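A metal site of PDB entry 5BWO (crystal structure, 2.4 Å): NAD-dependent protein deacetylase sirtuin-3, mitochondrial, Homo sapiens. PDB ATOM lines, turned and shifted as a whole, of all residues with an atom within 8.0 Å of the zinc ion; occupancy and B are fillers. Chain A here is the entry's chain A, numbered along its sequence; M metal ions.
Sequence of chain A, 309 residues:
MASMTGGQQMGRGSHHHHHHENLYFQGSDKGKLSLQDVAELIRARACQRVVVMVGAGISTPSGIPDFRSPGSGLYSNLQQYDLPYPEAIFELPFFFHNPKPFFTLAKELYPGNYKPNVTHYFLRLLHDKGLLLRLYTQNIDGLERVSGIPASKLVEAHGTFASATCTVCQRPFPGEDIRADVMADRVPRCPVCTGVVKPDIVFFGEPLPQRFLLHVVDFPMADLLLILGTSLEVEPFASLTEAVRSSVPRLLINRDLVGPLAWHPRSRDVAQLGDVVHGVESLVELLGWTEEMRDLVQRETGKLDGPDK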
ATOM      1  N   THR A 165       2.463 -16.442   8.948  1.00  0.00           N
ATOM      2  CA  THR A 165       2.994 -15.173   9.406  1.00  0.00           C
ATOM      3  C   THR A 165       2.012 -14.538  10.382  1.00  0.00           C
ATOM      4  O   THR A 165       0.806 -14.512  10.129  1.00  0.00           O
ATOM      5  CB  THR A 165       3.244 -14.216   8.232  1.00  0.00           C
ATOM      6  OG1 THR A 165       4.212 -14.793   7.346  1.00  0.00           O
ATOM      7  CG2 THR A 165       3.764 -12.864   8.726  1.00  0.00           C
ATOM      8  N   CYS A 166       2.541 -14.028  11.497  1.00  0.00           N
ATOM      9  CA  CYS A 166       1.706 -13.310  12.446  1.00  0.00           C
ATOM     10  C   CYS A 166       1.339 -11.940  11.890  1.00  0.00           C
ATOM     11  O   CYS A 166       2.208 -11.159  11.497  1.00  0.00           O
ATOM     12  CB  CYS A 166       2.428 -13.142  13.787  1.00  0.00           C
ATOM     13  SG  CYS A 166       1.484 -12.167  14.977  1.00  0.00           S
ATOM     14  N   THR A 167       0.039 -11.632  11.862  1.00  0.00           N
ATOM     15  CA  THR A 167      -0.454 -10.404  11.263  1.00  0.00           C
ATOM     16  C   THR A 167      -0.160  -9.167  12.118  1.00  0.00           C
ATOM     17  O   THR A 167      -0.404  -8.054  11.655  1.00  0.00           O
ATOM     18  CB  THR A 167      -1.963 -10.504  11.027  1.00  0.00           C
ATOM     19  OG1 THR A 167      -2.642 -10.715  12.271  1.00  0.00           O
ATOM     20  CG2 THR A 167      -2.274 -11.648  10.084  1.00  0.00           C
ATOM     21  N   VAL A 168       0.360  -9.347  13.333  1.00  0.00           N
ATOM     22  CA  VAL A 168       0.618  -8.239  14.262  1.00  0.00           C
ATOM     23  C   VAL A 168       2.104  -7.894  14.319  1.00  0.00           C
ATOM     24  O   VAL A 168       2.497  -6.750  14.061  1.00  0.00           O
ATOM     25  CB  VAL A 168       0.061  -8.540  15.664  1.00  0.00           C
ATOM     26  CG1 VAL A 168       0.382  -7.405  16.646  1.00  0.00           C
ATOM     27  CG2 VAL A 168      -1.448  -8.769  15.606  1.00  0.00           C
ATOM     28  N   CYS A 169       2.948  -8.860  14.654  1.00  0.00           N
ATOM     29  CA  CYS A 169       4.388  -8.644  14.756  1.00  0.00           C
ATOM     30  C   CYS A 169       5.160  -9.185  13.556  1.00  0.00           C
ATOM     31  O   CYS A 169       6.388  -9.079  13.529  1.00  0.00           O
ATOM     32  CB  CYS A 169       4.937  -9.251  16.051  1.00  0.00           C
ATOM     33  SG  CYS A 169       5.024 -11.048  16.085  1.00  0.00           S
ATOM     34  N   GLN A 170       4.468  -9.763  12.570  1.00  0.00           N
ATOM     35  CA  GLN A 170       5.070 -10.198  11.313  1.00  0.00           C
ATOM     36  C   GLN A 170       6.121 -11.284  11.502  1.00  0.00           C
ATOM     37  O   GLN A 170       6.969 -11.487  10.628  1.00  0.00           O
ATOM     38  CB  GLN A 170       5.677  -9.000  10.571  1.00  0.00           C
ATOM     39  CG  GLN A 170       4.634  -8.002  10.083  1.00  0.00           C
ATOM     40  CD  GLN A 170       3.649  -8.623   9.112  1.00  0.00           C
ATOM     41  OE1 GLN A 170       4.034  -9.408   8.242  1.00  0.00           O
ATOM     42  NE2 GLN A 170       2.376  -8.295   9.265  1.00  0.00           N
ATOM     43  N   ARG A 171       6.083 -11.992  12.616  1.00  0.00           N
ATOM     44  CA  ARG A 171       6.999 -13.106  12.807  1.00  0.00           C
ATOM     45  C   ARG A 171       6.556 -14.289  11.951  1.00  0.00           C
ATOM     46  O   ARG A 171       5.394 -14.692  12.016  1.00  0.00           O
ATOM     47  CB  ARG A 171       7.062 -13.500  14.282  1.00  0.00           C
ATOM     48  CG  ARG A 171       7.879 -14.762  14.548  1.00  0.00           C
ATOM     49  CD  ARG A 171       8.270 -14.890  16.019  1.00  0.00           C
ATOM     50  NE  ARG A 171       9.331 -13.955  16.397  1.00  0.00           N
ATOM     51  CZ  ARG A 171       9.137 -12.743  16.911  1.00  0.00           C
ATOM     52  NH1 ARG A 171      10.181 -11.982  17.208  1.00  0.00           N
ATOM     53  NH2 ARG A 171       7.911 -12.287  17.124  1.00  0.00           N
ATOM     54  N   PRO A 172       7.450 -14.864  11.142  1.00  0.00           N
ATOM     55  CA  PRO A 172       7.054 -16.037  10.344  1.00  0.00           C
ATOM     56  C   PRO A 172       7.172 -17.326  11.134  1.00  0.00           C
ATOM     57  O   PRO A 172       7.959 -17.448  12.079  1.00  0.00           O
ATOM     58  CB  PRO A 172       8.051 -16.004   9.180  1.00  0.00           C
ATOM     59  CG  PRO A 172       9.285 -15.436   9.790  1.00  0.00           C
ATOM     60  CD  PRO A 172       8.831 -14.446  10.845  1.00  0.00           C
ATOM     61  N   PHE A 173       6.378 -18.305  10.728  1.00  0.00           N
ATOM     62  CA  PHE A 173       6.353 -19.614  11.354  1.00  0.00           C
ATOM     63  C   PHE A 173       6.208 -20.672  10.271  1.00  0.00           C
ATOM     64  O   PHE A 173       5.749 -20.374   9.164  1.00  0.00           O
ATOM     65  CB  PHE A 173       5.201 -19.749  12.349  1.00  0.00           C
ATOM     66  CG  PHE A 173       5.272 -18.796  13.498  1.00  0.00           C
ATOM     67  CD1 PHE A 173       6.042 -19.085  14.616  1.00  0.00           C
ATOM     68  CD2 PHE A 173       4.570 -17.601  13.477  1.00  0.00           C
ATOM     69  CE1 PHE A 173       6.112 -18.205  15.681  1.00  0.00           C
ATOM     70  CE2 PHE A 173       4.640 -16.711  14.532  1.00  0.00           C
ATOM     71  CZ  PHE A 173       5.413 -17.013  15.638  1.00  0.00           C
ATOM     72  N   ARG A 189      -3.014 -18.474  17.357  1.00  0.00           N
ATOM     73  CA  ARG A 189      -2.497 -17.258  17.966  1.00  0.00           C
ATOM     74  C   ARG A 189      -0.971 -17.314  18.004  1.00  0.00           C
ATOM     75  O   ARG A 189      -0.367 -18.394  18.071  1.00  0.00           O
ATOM     76  CB  ARG A 189      -3.056 -17.087  19.385  1.00  0.00           C
ATOM     77  CG  ARG A 189      -4.565 -16.868  19.438  1.00  0.00           C
ATOM     78  CD  ARG A 189      -4.921 -15.454  19.027  1.00  0.00           C
ATOM     79  NE  ARG A 189      -6.368 -15.243  18.911  1.00  0.00           N
ATOM     80  CZ  ARG A 189      -6.919 -14.085  18.552  1.00  0.00           C
ATOM     81  NH1 ARG A 189      -6.159 -13.029  18.284  1.00  0.00           N
ATOM     82  NH2 ARG A 189      -8.236 -13.979  18.475  1.00  0.00           N
ATOM     83  N   CYS A 190      -0.350 -16.142  17.954  1.00  0.00           N
ATOM     84  CA  CYS A 190       1.107 -16.056  17.891  1.00  0.00           C
ATOM     85  C   CYS A 190       1.694 -16.304  19.283  1.00  0.00           C
ATOM     86  O   CYS A 190       1.261 -15.673  20.252  1.00  0.00           O
ATOM     87  CB  CYS A 190       1.531 -14.694  17.382  1.00  0.00           C
ATOM     88  SG  CYS A 190       3.320 -14.423  17.356  1.00  0.00           S
ATOM     89  N   PRO A 191       2.681 -17.192  19.422  1.00  0.00           N
ATOM     90  CA  PRO A 191       3.274 -17.428  20.749  1.00  0.00           C
ATOM     91  C   PRO A 191       3.998 -16.216  21.309  1.00  0.00           C
ATOM     92  O   PRO A 191       4.242 -16.180  22.526  1.00  0.00           O
ATOM     93  CB  PRO A 191       4.245 -18.588  20.499  1.00  0.00           C
ATOM     94  CG  PRO A 191       4.567 -18.529  19.047  1.00  0.00           C
ATOM     95  CD  PRO A 191       3.329 -18.015  18.377  1.00  0.00           C
ATOM     96  N   VAL A 192       4.336 -15.231  20.486  1.00  0.00           N
ATOM     97  CA  VAL A 192       5.069 -14.054  20.948  1.00  0.00           C
ATOM     98  C   VAL A 192       4.115 -12.926  21.350  1.00  0.00           C
ATOM     99  O   VAL A 192       4.194 -12.416  22.471  1.00  0.00           O
ATOM    100  CB  VAL A 192       6.071 -13.597  19.871  1.00  0.00           C
ATOM    101  CG1 VAL A 192       6.776 -12.318  20.301  1.00  0.00           C
ATOM    102  CG2 VAL A 192       7.098 -14.692  19.613  1.00  0.00           C
ATOM    103  N   CYS A 193       3.221 -12.516  20.456  1.00  0.00           N
ATOM    104  CA  CYS A 193       2.306 -11.415  20.739  1.00  0.00           C
ATOM    105  C   CYS A 193       0.838 -11.820  20.770  1.00  0.00           C
ATOM    106  O   CYS A 193      -0.018 -10.962  20.978  1.00  0.00           O
ATOM    107  CB  CYS A 193       2.493 -10.282  19.706  1.00  0.00           C
ATOM    108  SG  CYS A 193       1.837 -10.623  18.066  1.00  0.00           S
ATOM    109  N   THR A 194       0.521 -13.103  20.589  1.00  0.00           N
ATOM    110  CA  THR A 194      -0.840 -13.626  20.572  1.00  0.00           C
ATOM    111  C   THR A 194      -1.660 -13.101  19.400  1.00  0.00           C
ATOM    112  O   THR A 194      -2.866 -13.354  19.333  1.00  0.00           O
ATOM    113  CB  THR A 194      -1.605 -13.322  21.862  1.00  0.00           C
ATOM    114  OG1 THR A 194      -1.912 -11.925  21.941  1.00  0.00           O
ATOM    115  CG2 THR A 194      -0.795 -13.752  23.091  1.00  0.00           C
ATOM    116  N   GLY A 195      -1.041 -12.366  18.468  1.00  0.00           N
ATOM    117  CA  GLY A 195      -1.749 -11.968  17.277  1.00  0.00           C
ATOM    118  C   GLY A 195      -2.198 -13.158  16.444  1.00  0.00           C
ATOM    119  O   GLY A 195      -1.744 -14.290  16.624  1.00  0.00           O
ATOM    120  N   VAL A 196      -3.121 -12.889  15.526  1.00  0.00           N
ATOM    121  CA  VAL A 196      -3.621 -13.947  14.659  1.00  0.00           C
ATOM    122  C   VAL A 196      -2.538 -14.342  13.672  1.00  0.00           C
ATOM    123  O   VAL A 196      -1.942 -13.485  12.992  1.00  0.00           O
ATOM    124  CB  VAL A 196      -4.902 -13.488  13.929  1.00  0.00           C
ATOM    125  CG1 VAL A 196      -5.347 -14.530  12.906  1.00  0.00           C
ATOM    126  CG2 VAL A 196      -6.002 -13.236  14.931  1.00  0.00           C
ATOM    127  N   VAL A 197      -2.246 -15.636  13.599  1.00  0.00           N
ATOM    128  CA  VAL A 197      -1.284 -16.175  12.651  1.00  0.00           C
ATOM    129  C   VAL A 197      -2.020 -16.514  11.366  1.00  0.00           C
ATOM    130  O   VAL A 197      -2.981 -17.281  11.378  1.00  0.00           O
ATOM    131  CB  VAL A 197      -0.562 -17.403  13.224  1.00  0.00           C
ATOM    132  CG1 VAL A 197       0.475 -17.928  12.251  1.00  0.00           C
ATOM    133  CG2 VAL A 197       0.078 -17.067  14.563  1.00  0.00           C
HETATM  134 ZN    ZN M   1       3.138 -12.177  16.736  1.00  0.00          ZN
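The guanidinium group of Arg 171 sits close to the side-chain sulfur of Cys 169 (3.3 Å). The side-chain sulfur (SG) of Cys 190 sits close to the backbone NH (N) of Val 192 (3.4 Å). The backbone NH (N) of Cys 190 is in hydrogen-bond range of the backbone carbonyl oxygen (O) of Gly 195 (2.7 Å). The backbone NH of Cys 166 sits at hydrogen-bond distance from the backbone carbonyl oxygen of Arg 171 (3.0 Å). N of Val 168 sits close to SG of Cys 166 (3.5 Å). The side-chain sulfur (SG) of Cys 193 lies close to the backbone NH (N) of Gly 195 (3.4 Å).
Of the 18 residues printed, 4 come within 4 Å of the zinc ion. The nearest printed residue that does not touch the zinc ion is Val 192 (4.5 Å).
The zinc ion is bound by SG of Cys 169 (2.3 Å), SG of Cys 190 (2.3 Å), SG of Cys 166 (2.4 Å) and SG of Cys 193 (2.4 Å). The zinc ion has four donor atoms within binding distance.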
